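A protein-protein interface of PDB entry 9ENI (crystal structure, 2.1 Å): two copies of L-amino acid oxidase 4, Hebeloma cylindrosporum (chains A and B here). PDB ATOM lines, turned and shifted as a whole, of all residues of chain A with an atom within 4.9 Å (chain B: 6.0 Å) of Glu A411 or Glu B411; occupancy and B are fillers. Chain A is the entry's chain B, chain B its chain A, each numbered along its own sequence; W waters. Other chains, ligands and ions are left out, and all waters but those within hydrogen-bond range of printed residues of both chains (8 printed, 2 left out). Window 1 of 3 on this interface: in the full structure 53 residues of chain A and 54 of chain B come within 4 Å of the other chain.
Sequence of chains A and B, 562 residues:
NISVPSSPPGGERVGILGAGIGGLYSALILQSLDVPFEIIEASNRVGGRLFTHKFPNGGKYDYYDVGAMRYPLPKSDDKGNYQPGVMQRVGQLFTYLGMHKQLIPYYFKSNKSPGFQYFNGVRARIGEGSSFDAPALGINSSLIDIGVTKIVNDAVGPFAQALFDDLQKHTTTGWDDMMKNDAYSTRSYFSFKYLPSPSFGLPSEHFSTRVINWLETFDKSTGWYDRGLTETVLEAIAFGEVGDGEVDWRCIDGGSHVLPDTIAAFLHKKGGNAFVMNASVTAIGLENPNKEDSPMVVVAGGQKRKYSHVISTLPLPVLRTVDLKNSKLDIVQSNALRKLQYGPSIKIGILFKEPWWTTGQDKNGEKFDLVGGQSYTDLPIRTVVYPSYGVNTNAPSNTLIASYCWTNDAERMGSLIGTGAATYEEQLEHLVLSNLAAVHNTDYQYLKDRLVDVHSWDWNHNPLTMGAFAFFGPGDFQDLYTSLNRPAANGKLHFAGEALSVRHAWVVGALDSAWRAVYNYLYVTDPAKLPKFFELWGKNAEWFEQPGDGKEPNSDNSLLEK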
ATOM      1  N   ARG A 227      -7.448  25.930  28.393  1.00  0.00           N
ATOM      2  CA  ARG A 227      -8.524  25.863  29.366  1.00  0.00           C
ATOM      3  C   ARG A 227      -8.207  26.811  30.523  1.00  0.00           C
ATOM      4  O   ARG A 227      -7.196  27.516  30.519  1.00  0.00           O
ATOM      5  CB  ARG A 227      -8.735  24.411  29.790  1.00  0.00           C
ATOM      6  CG  ARG A 227      -9.350  23.597  28.651  1.00  0.00           C
ATOM      7  CD  ARG A 227      -9.313  22.111  28.861  1.00  0.00           C
ATOM      8  NE  ARG A 227      -9.732  21.403  27.655  1.00  0.00           N
ATOM      9  CZ  ARG A 227     -10.954  20.930  27.441  1.00  0.00           C
ATOM     10  NH1 ARG A 227     -11.925  21.091  28.324  1.00  0.00           N
ATOM     11  NH2 ARG A 227     -11.210  20.277  26.312  1.00  0.00           N
ATOM     12  N   PRO A 344     -11.586  15.547  27.616  1.00  0.00           N
ATOM     13  CA  PRO A 344     -11.534  14.156  27.164  1.00  0.00           C
ATOM     14  C   PRO A 344     -10.348  13.423  27.777  1.00  0.00           C
ATOM     15  O   PRO A 344      -9.448  14.022  28.366  1.00  0.00           O
ATOM     16  CB  PRO A 344     -11.358  14.307  25.653  1.00  0.00           C
ATOM     17  CG  PRO A 344     -10.472  15.535  25.548  1.00  0.00           C
ATOM     18  CD  PRO A 344     -10.856  16.441  26.697  1.00  0.00           C
ATOM     19  N   THR A 407      -6.865  16.138  26.719  1.00  0.00           N
ATOM     20  CA  THR A 407      -7.096  17.217  25.760  1.00  0.00           C
ATOM     21  C   THR A 407      -6.878  16.763  24.317  1.00  0.00           C
ATOM     22  O   THR A 407      -7.391  15.709  23.930  1.00  0.00           O
ATOM     23  CB  THR A 407      -6.215  18.416  26.130  1.00  0.00           C
ATOM     24  OG1 THR A 407      -4.847  18.006  26.246  1.00  0.00           O
ATOM     25  CG2 THR A 407      -6.659  18.998  27.468  1.00  0.00           C
ATOM     26  N   ASN A 408      -6.145  17.540  23.509  1.00  0.00           N
ATOM     27  CA  ASN A 408      -6.053  17.241  22.079  1.00  0.00           C
ATOM     28  C   ASN A 408      -5.492  15.842  21.827  1.00  0.00           C
ATOM     29  O   ASN A 408      -5.899  15.163  20.876  1.00  0.00           O
ATOM     30  CB  ASN A 408      -5.174  18.267  21.359  1.00  0.00           C
ATOM     31  CG  ASN A 408      -5.739  19.680  21.385  1.00  0.00           C
ATOM     32  OD1 ASN A 408      -4.985  20.643  21.253  1.00  0.00           O
ATOM     33  ND2 ASN A 408      -7.052  19.813  21.547  1.00  0.00           N
ATOM     34  N   ASP A 409      -4.526  15.412  22.641  1.00  0.00           N
ATOM     35  CA  ASP A 409      -3.921  14.101  22.430  1.00  0.00           C
ATOM     36  C   ASP A 409      -4.967  13.000  22.554  1.00  0.00           C
ATOM     37  O   ASP A 409      -4.955  12.025  21.792  1.00  0.00           O
ATOM     38  CB  ASP A 409      -2.790  13.875  23.435  1.00  0.00           C
ATOM     39  CG  ASP A 409      -1.765  14.996  23.430  1.00  0.00           C
ATOM     40  OD1 ASP A 409      -1.266  15.353  22.342  1.00  0.00           O
ATOM     41  OD2 ASP A 409      -1.468  15.527  24.522  1.00  0.00           O
ATOM     42  N   ALA A 410      -5.885  13.150  23.513  1.00  0.00           N
ATOM     43  CA  ALA A 410      -6.953  12.175  23.694  1.00  0.00           C
ATOM     44  C   ALA A 410      -7.993  12.287  22.587  1.00  0.00           C
ATOM     45  O   ALA A 410      -8.531  11.272  22.131  1.00  0.00           O
ATOM     46  CB  ALA A 410      -7.607  12.371  25.062  1.00  0.00           C
ATOM     47  N   GLU A 411      -8.294  13.512  22.150  1.00  0.00           N
ATOM     48  CA  GLU A 411      -9.253  13.699  21.064  1.00  0.00           C
ATOM     49  C   GLU A 411      -8.773  13.013  19.792  1.00  0.00           C
ATOM     50  O   GLU A 411      -9.534  12.300  19.128  1.00  0.00           O
ATOM     51  CB  GLU A 411      -9.481  15.194  20.824  1.00  0.00           C
ATOM     52  CG  GLU A 411     -10.191  15.881  21.982  1.00  0.00           C
ATOM     53  CD  GLU A 411      -9.984  17.387  22.018  1.00  0.00           C
ATOM     54  OE1 GLU A 411      -9.234  17.919  21.170  1.00  0.00           O
ATOM     55  OE2 GLU A 411     -10.562  18.035  22.919  1.00  0.00           O
ATOM     56  N   ARG A 412      -7.502  13.215  19.441  1.00  0.00           N
ATOM     57  CA  ARG A 412      -6.962  12.608  18.231  1.00  0.00           C
ATOM     58  C   ARG A 412      -6.904  11.090  18.358  1.00  0.00           C
ATOM     59  O   ARG A 412      -7.391  10.367  17.481  1.00  0.00           O
ATOM     60  CB  ARG A 412      -5.580  13.193  17.930  1.00  0.00           C
ATOM     61  CG  ARG A 412      -5.599  14.695  17.612  1.00  0.00           C
ATOM     62  CD  ARG A 412      -4.199  15.228  17.365  1.00  0.00           C
ATOM     63  NE  ARG A 412      -4.203  16.553  16.752  1.00  0.00           N
ATOM     64  CZ  ARG A 412      -3.183  17.069  16.077  1.00  0.00           C
ATOM     65  NH1 ARG A 412      -2.055  16.398  15.909  1.00  0.00           N
ATOM     66  NH2 ARG A 412      -3.302  18.282  15.547  1.00  0.00           N
ATOM     67  N   MET A 413      -6.321  10.583  19.449  1.00  0.00           N
ATOM     68  CA  MET A 413      -6.223   9.136  19.615  1.00  0.00           C
ATOM     69  C   MET A 413      -7.597   8.481  19.658  1.00  0.00           C
ATOM     70  O   MET A 413      -7.749   7.324  19.249  1.00  0.00           O
ATOM     71  CB  MET A 413      -5.450   8.796  20.889  1.00  0.00           C
ATOM     72  CG  MET A 413      -5.065   7.329  20.984  1.00  0.00           C
ATOM     73  SD  MET A 413      -3.737   6.912  19.838  1.00  0.00           S
ATOM     74  CE  MET A 413      -2.303   7.357  20.817  1.00  0.00           C
ATOM     75  N   GLY A 414      -8.607   9.199  20.149  1.00  0.00           N
ATOM     76  CA  GLY A 414      -9.929   8.612  20.271  1.00  0.00           C
ATOM     77  C   GLY A 414     -10.485   8.098  18.960  1.00  0.00           C
ATOM     78  O   GLY A 414     -11.282   7.154  18.947  1.00  0.00           O
ATOM     79  N   SER A 415     -10.073   8.695  17.840  1.00  0.00           N
ATOM     80  CA  SER A 415     -10.607   8.268  16.555  1.00  0.00           C
ATOM     81  C   SER A 415     -10.198   6.848  16.205  1.00  0.00           C
ATOM     82  O   SER A 415     -10.881   6.206  15.404  1.00  0.00           O
ATOM     83  CB  SER A 415     -10.155   9.219  15.444  1.00  0.00           C
ATOM     84  OG  SER A 415     -11.029  10.327  15.328  1.00  0.00           O
ATOM     85  N   ASN A 460     -14.466  10.022  26.120  1.00  0.00           N
ATOM     86  CA  ASN A 460     -15.187  10.988  25.302  1.00  0.00           C
ATOM     87  C   ASN A 460     -16.007  10.326  24.196  1.00  0.00           C
ATOM     88  O   ASN A 460     -16.463  11.011  23.274  1.00  0.00           O
ATOM     89  CB  ASN A 460     -14.214  11.995  24.693  1.00  0.00           C
ATOM     90  CG  ASN A 460     -14.884  13.300  24.335  1.00  0.00           C
ATOM     91  OD1 ASN A 460     -15.823  13.737  25.004  1.00  0.00           O
ATOM     92  ND2 ASN A 460     -14.415  13.926  23.268  1.00  0.00           N
ATOM     93  N   ARG B 227     -11.086  29.195  21.415  1.00  0.00           N
ATOM     94  CA  ARG B 227     -10.097  29.002  20.374  1.00  0.00           C
ATOM     95  C   ARG B 227      -9.636  30.365  19.868  1.00  0.00           C
ATOM     96  O   ARG B 227     -10.040  31.413  20.376  1.00  0.00           O
ATOM     97  CB  ARG B 227     -10.673  28.108  19.282  1.00  0.00           C
ATOM     98  CG  ARG B 227     -10.820  26.676  19.779  1.00  0.00           C
ATOM     99  CD  ARG B 227     -11.667  25.839  18.872  1.00  0.00           C
ATOM    100  NE  ARG B 227     -11.979  24.547  19.472  1.00  0.00           N
ATOM    101  CZ  ARG B 227     -11.358  23.406  19.198  1.00  0.00           C
ATOM    102  NH1 ARG B 227     -10.356  23.349  18.332  1.00  0.00           N
ATOM    103  NH2 ARG B 227     -11.768  22.289  19.794  1.00  0.00           N
ATOM    104  N   GLN B 341      -4.222  22.949  16.260  1.00  0.00           N
ATOM    105  CA  GLN B 341      -5.394  22.308  16.835  1.00  0.00           C
ATOM    106  C   GLN B 341      -6.468  22.038  15.793  1.00  0.00           C
ATOM    107  O   GLN B 341      -6.731  22.860  14.912  1.00  0.00           O
ATOM    108  CB  GLN B 341      -5.978  23.177  17.953  1.00  0.00           C
ATOM    109  CG  GLN B 341      -6.987  22.442  18.808  1.00  0.00           C
ATOM    110  CD  GLN B 341      -7.497  23.254  19.988  1.00  0.00           C
ATOM    111  OE1 GLN B 341      -7.844  22.694  21.020  1.00  0.00           O
ATOM    112  NE2 GLN B 341      -7.572  24.571  19.829  1.00  0.00           N
ATOM    113  N   TYR B 342      -7.122  20.891  15.936  1.00  0.00           N
ATOM    114  CA  TYR B 342      -8.284  20.518  15.144  1.00  0.00           C
ATOM    115  C   TYR B 342      -9.548  20.685  15.979  1.00  0.00           C
ATOM    116  O   TYR B 342      -9.507  20.730  17.211  1.00  0.00           O
ATOM    117  CB  TYR B 342      -8.158  19.074  14.641  1.00  0.00           C
ATOM    118  CG  TYR B 342      -7.436  18.969  13.313  1.00  0.00           C
ATOM    119  CD1 TYR B 342      -6.154  19.481  13.156  1.00  0.00           C
ATOM    120  CD2 TYR B 342      -8.041  18.373  12.213  1.00  0.00           C
ATOM    121  CE1 TYR B 342      -5.494  19.406  11.943  1.00  0.00           C
ATOM    122  CE2 TYR B 342      -7.389  18.292  10.994  1.00  0.00           C
ATOM    123  CZ  TYR B 342      -6.115  18.811  10.867  1.00  0.00           C
ATOM    124  OH  TYR B 342      -5.454  18.737   9.664  1.00  0.00           O
ATOM    125  N   PRO B 344     -13.909  19.580  16.392  1.00  0.00           N
ATOM    126  CA  PRO B 344     -14.847  18.483  16.147  1.00  0.00           C
ATOM    127  C   PRO B 344     -16.106  18.942  15.422  1.00  0.00           C
ATOM    128  O   PRO B 344     -16.398  20.135  15.313  1.00  0.00           O
ATOM    129  CB  PRO B 344     -15.193  18.024  17.566  1.00  0.00           C
ATOM    130  CG  PRO B 344     -15.195  19.313  18.344  1.00  0.00           C
ATOM    131  CD  PRO B 344     -14.131  20.198  17.714  1.00  0.00           C
ATOM    132  N   ILE B 346     -20.260  16.983  14.363  1.00  0.00           N
ATOM    133  CA  ILE B 346     -21.146  15.858  14.100  1.00  0.00           C
ATOM    134  C   ILE B 346     -22.310  16.350  13.253  1.00  0.00           C
ATOM    135  O   ILE B 346     -22.667  17.532  13.273  1.00  0.00           O
ATOM    136  CB  ILE B 346     -21.679  15.189  15.388  1.00  0.00           C
ATOM    137  CG1 ILE B 346     -22.658  16.109  16.120  1.00  0.00           C
ATOM    138  CG2 ILE B 346     -20.536  14.807  16.299  1.00  0.00           C
ATOM    139  CD1 ILE B 346     -24.139  15.893  15.745  1.00  0.00           C
ATOM    140  N   TRP B 406     -20.784  21.877  16.563  1.00  0.00           N
ATOM    141  CA  TRP B 406     -19.370  22.202  16.633  1.00  0.00           C
ATOM    142  C   TRP B 406     -18.887  22.102  18.079  1.00  0.00           C
ATOM    143  O   TRP B 406     -19.679  21.962  19.017  1.00  0.00           O
ATOM    144  CB  TRP B 406     -19.102  23.620  16.105  1.00  0.00           C
ATOM    145  CG  TRP B 406     -19.457  23.836  14.667  1.00  0.00           C
ATOM    146  CD1 TRP B 406     -19.367  22.929  13.652  1.00  0.00           C
ATOM    147  CD2 TRP B 406     -19.954  25.046  14.081  1.00  0.00           C
ATOM    148  NE1 TRP B 406     -19.780  23.497  12.471  1.00  0.00           N
ATOM    149  CE2 TRP B 406     -20.143  24.796  12.708  1.00  0.00           C
ATOM    150  CE3 TRP B 406     -20.254  26.314  14.584  1.00  0.00           C
ATOM    151  CZ2 TRP B 406     -20.623  25.772  11.831  1.00  0.00           C
ATOM    152  CZ3 TRP B 406     -20.721  27.283  13.711  1.00  0.00           C
ATOM    153  CH2 TRP B 406     -20.911  27.003  12.353  1.00  0.00           C
ATOM    154  N   THR B 407     -17.563  22.181  18.238  1.00  0.00           N
ATOM    155  CA  THR B 407     -16.895  22.303  19.534  1.00  0.00           C
ATOM    156  C   THR B 407     -17.549  21.442  20.616  1.00  0.00           C
ATOM    157  O   THR B 407     -17.787  20.251  20.386  1.00  0.00           O
ATOM    158  CB  THR B 407     -16.830  23.785  19.936  1.00  0.00           C
ATOM    159  OG1 THR B 407     -18.137  24.372  19.893  1.00  0.00           O
ATOM    160  CG2 THR B 407     -15.915  24.554  18.968  1.00  0.00           C
ATOM    161  N   ASN B 408     -17.802  22.005  21.807  1.00  0.00           N
ATOM    162  CA  ASN B 408     -18.264  21.187  22.929  1.00  0.00           C
ATOM    163  C   ASN B 408     -19.564  20.460  22.597  1.00  0.00           C
ATOM    164  O   ASN B 408     -19.787  19.332  23.051  1.00  0.00           O
ATOM    165  CB  ASN B 408     -18.472  22.031  24.189  1.00  0.00           C
ATOM    166  CG  ASN B 408     -17.193  22.648  24.724  1.00  0.00           C
ATOM    167  OD1 ASN B 408     -17.252  23.652  25.432  1.00  0.00           O
ATOM    168  ND2 ASN B 408     -16.041  22.065  24.395  1.00  0.00           N
ATOM    169  N   ASP B 409     -20.458  21.110  21.848  1.00  0.00           N
ATOM    170  CA  ASP B 409     -21.729  20.475  21.514  1.00  0.00           C
ATOM    171  C   ASP B 409     -21.504  19.201  20.707  1.00  0.00           C
ATOM    172  O   ASP B 409     -22.185  18.188  20.922  1.00  0.00           O
ATOM    173  CB  ASP B 409     -22.620  21.448  20.740  1.00  0.00           C
ATOM    174  CG  ASP B 409     -22.820  22.767  21.465  1.00  0.00           C
ATOM    175  OD1 ASP B 409     -23.179  22.743  22.665  1.00  0.00           O
ATOM    176  OD2 ASP B 409     -22.618  23.828  20.832  1.00  0.00           O
ATOM    177  N   ALA B 410     -20.546  19.229  19.776  1.00  0.00           N
ATOM    178  CA  ALA B 410     -20.248  18.042  18.981  1.00  0.00           C
ATOM    179  C   ALA B 410     -19.516  16.991  19.807  1.00  0.00           C
ATOM    180  O   ALA B 410     -19.756  15.790  19.644  1.00  0.00           O
ATOM    181  CB  ALA B 410     -19.424  18.424  17.750  1.00  0.00           C
ATOM    182  N   GLU B 411     -18.617  17.421  20.697  1.00  0.00           N
ATOM    183  CA  GLU B 411     -17.909  16.472  21.552  1.00  0.00           C
ATOM    184  C   GLU B 411     -18.884  15.699  22.426  1.00  0.00           C
ATOM    185  O   GLU B 411     -18.787  14.472  22.555  1.00  0.00           O
ATOM    186  CB  GLU B 411     -16.883  17.213  22.409  1.00  0.00           C
ATOM    187  CG  GLU B 411     -15.759  17.804  21.581  1.00  0.00           C
ATOM    188  CD  GLU B 411     -15.044  18.926  22.283  1.00  0.00           C
ATOM    189  OE1 GLU B 411     -15.458  19.285  23.407  1.00  0.00           O
ATOM    190  OE2 GLU B 411     -14.082  19.470  21.698  1.00  0.00           O
ATOM    191  N   ARG B 412     -19.832  16.405  23.043  1.00  0.00           N
ATOM    192  CA  ARG B 412     -20.806  15.730  23.890  1.00  0.00           C
ATOM    193  C   ARG B 412     -21.699  14.811  23.065  1.00  0.00           C
ATOM    194  O   ARG B 412     -21.832  13.621  23.373  1.00  0.00           O
ATOM    195  CB  ARG B 412     -21.637  16.763  24.652  1.00  0.00           C
ATOM    196  CG  ARG B 412     -20.820  17.608  25.616  1.00  0.00           C
ATOM    197  CD  ARG B 412     -21.682  18.640  26.302  1.00  0.00           C
ATOM    198  NE  ARG B 412     -21.005  19.234  27.447  1.00  0.00           N
ATOM    199  CZ  ARG B 412     -21.626  19.834  28.452  1.00  0.00           C
ATOM    200  NH1 ARG B 412     -22.945  19.932  28.492  1.00  0.00           N
ATOM    201  NH2 ARG B 412     -20.906  20.337  29.448  1.00  0.00           N
ATOM    202  N   MET B 413     -22.293  15.331  21.988  1.00  0.00           N
ATOM    203  CA  MET B 413     -23.184  14.502  21.181  1.00  0.00           C
ATOM    204  C   MET B 413     -22.454  13.293  20.600  1.00  0.00           C
ATOM    205  O   MET B 413     -23.071  12.244  20.378  1.00  0.00           O
ATOM    206  CB  MET B 413     -23.803  15.326  20.053  1.00  0.00           C
ATOM    207  CG  MET B 413     -24.968  14.627  19.352  1.00  0.00           C
ATOM    208  SD  MET B 413     -26.474  14.588  20.353  1.00  0.00           S
ATOM    209  CE  MET B 413     -27.210  16.173  19.951  1.00  0.00           C
ATOM    210  N   GLY B 414     -21.149  13.420  20.345  1.00  0.00           N
ATOM    211  CA  GLY B 414     -20.410  12.320  19.745  1.00  0.00           C
ATOM    212  C   GLY B 414     -20.469  11.039  20.553  1.00  0.00           C
ATOM    213  O   GLY B 414     -20.381   9.943  19.991  1.00  0.00           O
ATOM    214  N   SER B 415     -20.628  11.151  21.875  1.00  0.00           N
ATOM    215  CA  SER B 415     -20.665   9.957  22.712  1.00  0.00           C
ATOM    216  C   SER B 415     -21.874   9.082  22.417  1.00  0.00           C
ATOM    217  O   SER B 415     -21.871   7.903  22.785  1.00  0.00           O
ATOM    218  CB  SER B 415     -20.651  10.335  24.193  1.00  0.00           C
ATOM    219  OG  SER B 415     -19.325  10.481  24.666  1.00  0.00           O
ATOM    220  N   ASP B 458     -19.725  11.264  13.222  1.00  0.00           N
ATOM    221  CA  ASP B 458     -18.857  11.999  14.138  1.00  0.00           C
ATOM    222  C   ASP B 458     -17.475  12.091  13.499  1.00  0.00           C
ATOM    223  O   ASP B 458     -16.703  11.126  13.528  1.00  0.00           O
ATOM    224  CB  ASP B 458     -18.799  11.308  15.496  1.00  0.00           C
ATOM    225  CG  ASP B 458     -17.932  12.048  16.498  1.00  0.00           C
ATOM    226  OD1 ASP B 458     -17.372  13.111  16.155  1.00  0.00           O
ATOM    227  OD2 ASP B 458     -17.812  11.553  17.636  1.00  0.00           O
ATOM    228  N   ASN B 460     -14.995  13.487  14.598  1.00  0.00           N
ATOM    229  CA  ASN B 460     -13.979  13.345  15.631  1.00  0.00           C
ATOM    230  C   ASN B 460     -13.851  11.912  16.133  1.00  0.00           C
ATOM    231  O   ASN B 460     -13.123  11.667  17.102  1.00  0.00           O
ATOM    232  CB  ASN B 460     -14.271  14.281  16.801  1.00  0.00           C
ATOM    233  CG  ASN B 460     -13.034  14.591  17.601  1.00  0.00           C
ATOM    234  OD1 ASN B 460     -11.930  14.654  17.054  1.00  0.00           O
ATOM    235  ND2 ASN B 460     -13.201  14.764  18.906  1.00  0.00           N
ATOM    236  N   HIS B 461     -14.559  10.969  15.510  1.00  0.00           N
ATOM    237  CA  HIS B 461     -14.343   9.547  15.734  1.00  0.00           C
ATOM    238  C   HIS B 461     -14.347   8.871  14.360  1.00  0.00           C
ATOM    239  O   HIS B 461     -15.244   8.111  13.999  1.00  0.00           O
ATOM    240  CB  HIS B 461     -15.381   8.971  16.692  1.00  0.00           C
ATOM    241  CG  HIS B 461     -15.183   9.424  18.103  1.00  0.00           C
ATOM    242  ND1 HIS B 461     -15.723  10.594  18.590  1.00  0.00           N
ATOM    243  CD2 HIS B 461     -14.462   8.891  19.117  1.00  0.00           C
ATOM    244  CE1 HIS B 461     -15.366  10.750  19.852  1.00  0.00           C
ATOM    245  NE2 HIS B 461     -14.598   9.732  20.195  1.00  0.00           N
ATOM    246  N   MET B 466      -9.778  12.199  11.962  1.00  0.00           N
ATOM    247  CA  MET B 466      -9.292  12.435  13.322  1.00  0.00           C
ATOM    248  C   MET B 466      -9.611  13.861  13.768  1.00  0.00           C
ATOM    249  O   MET B 466      -8.779  14.572  14.336  1.00  0.00           O
ATOM    250  CB  MET B 466      -7.797  12.130  13.414  1.00  0.00           C
ATOM    251  CG  MET B 466      -7.456  10.699  13.005  1.00  0.00           C
ATOM    252  SD  MET B 466      -5.704  10.278  13.154  1.00  0.00           S
ATOM    253  CE  MET B 466      -5.545  10.050  14.925  1.00  0.00           C
HETATM  254  O   HOH W   1     -13.118  16.901  23.832  1.00  0.00           O
HETATM  255  O   HOH W   2     -10.373  19.886  19.768  1.00  0.00           O
HETATM  256  O   HOH W   3     -11.739  20.410  22.999  1.00  0.00           O
HETATM  257  O   HOH W   4     -12.281  17.752  20.121  1.00  0.00           O
HETATM  258  O   HOH W   5     -17.360  12.602  21.321  1.00  0.00           O
HETATM  259  O   HOH W   6     -12.001  11.169  19.510  1.00  0.00           O
HETATM  260  O   HOH W   7     -13.700  19.226  25.496  1.00  0.00           O
HETATM  261  O   HOH W   8      -5.971  18.887  17.484  1.00  0.00           O
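NH1 of Arg B227 lies close to NE2 of Gln B341 (3.4 Å).
The backbone carbonyl oxygen (O) of Tyr B342 lies within hydrogen-bond range of the guanidinium group (NH1) of Arg B227 (3.0 Å).
The side-chain carboxylate of Glu B411 is in hydrogen-bond range of the side-chain amide nitrogen of Asn B408, 3.0 Å away.
The backbone NH (N) of Asn B460 is in hydrogen-bond range of the side-chain carboxylate (OD1) of Asp B458, 2.9 Å away.
ND1 of His B461 is in hydrogen-bond range of OD2 of Asp B458 (2.5 Å).
The side-chain carboxylate of Glu A411 lies within hydrogen-bond range of the side-chain amide nitrogen of Asn A408, at 2.9 Å.
Water W3 lies within hydrogen-bond range of the side-chain carboxylate of Glu A411 (2.7 Å), the side-chain carboxylate of Glu B411 (2.8 Å) and the guanidinium group of Arg A227 (3.4 Å).
Water W5 lies within hydrogen-bond range of O of Glu B411 and O of Asn A460.
Water W2 lies within hydrogen-bond range of OE1 of Glu A411, NH2 of Arg B227 and O of Tyr B342.
Water W6 lies within hydrogen-bond range of the backbone carbonyl oxygen (O) of Asn B460 (2.7 Å), the backbone carbonyl oxygen (O) of Glu A411 (2.7 Å) and a ring nitrogen (NE2) of His B461 (3.0 Å).
Water W7 lies within hydrogen-bond range of the side-chain carboxylate of Glu B411 (2.7 Å) and the guanidinium group of Arg A227 (2.8 Å).
Water W4 lies within hydrogen-bond range of OE2 of Glu B411 (2.9 Å), OE1 of Glu A411 (3.2 Å) and ND2 of Asn B460 (3.4 Å).
OE1 of Gln B341 sits at hydrogen-bond distance from ND2 of Asn A408 (3.0 Å).
The backbone carbonyl oxygen (O) of Asn A460 lies within hydrogen-bond range of the side-chain hydroxyl (OG) of Ser B415 (3.2 Å).
O of Asn B460 is in hydrogen-bond range of OG of Ser A415 (3.1 Å).
Glu A411 touches its own counterpart, Glu B411.
Glu A411 touches Asn B460, and with the chains exchanged Asn A460 touches Glu B411.
Ser A415 touches Asn B460, and with the chains exchanged Asn A460 touches Ser B415.
12 positions are printed for both chains.
Of the 12 pairs that touch across the chains among the printed residues, 5 have their exchanged pair printed and touching as well.
Among the printed residues, merely in contact across the chains: Arg A412 with Met B466 (3.2 Å), Ser A415 with Met B466 (3.4 Å), Ser A415 with His B461 (3.4 Å), Asn A460 with His B461 (3.6 Å), Gly A414 with His B461 (3.6 Å), Arg A412 with Tyr B342 (3.9 Å), Asn A460 with Glu B411 (3.9 Å), Glu A411 with Asn B460 (3.9 Å) and Glu A411 with Glu B411 (3.99 Å).
Of the 12 printed residues of chain A, 6 touch a printed residue of chain B.
Printed residues of chain A that touch a printed residue of chain B: Asn A408, Glu A411, Arg A412, Gly A414, Ser A415 and Asn A460.
Of the 19 printed residues of chain B, 7 touch a printed residue of chain A.
Printed residues of chain B that touch a printed residue of chain A: Gln B341, Tyr B342, Glu B411, Ser B415, Asn B460, His B461 and Met B466.
Printed residues of chain B within 4 Å of Glu A411: Glu B411 (3.99 Å) and Asn B460 (3.9 Å).
Printed residues of chain B within 4 Å of Asn A460: Glu B411, Ser B415 and His B461.
Printed residues of chain A within 4 Å of Gln B341: Asn A408.
Of the printed residues of chain A, Tyr B342 touches Arg A412.
Ala B410 touches none of the printed residues of chain A.
Of the printed residues of chain A, Glu B411 touches Glu A411 (3.99 Å) and Asn A460 (3.9 Å).
Met B413 touches none of the printed residues of chain A.
Of the printed residues of chain A, Asn B460 touches Glu A411 (3.9 Å) and Ser A415 (3.1 Å).
Of the printed residues of chain A, Met B466 touches Arg A412 and Ser A415.
The nearest printed residue of chain A that does not touch Glu B411 is Arg A227 (5.2 Å).
The nearest printed residue of chain B that does not touch Arg A412 is Gln B341 (4.7 Å).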
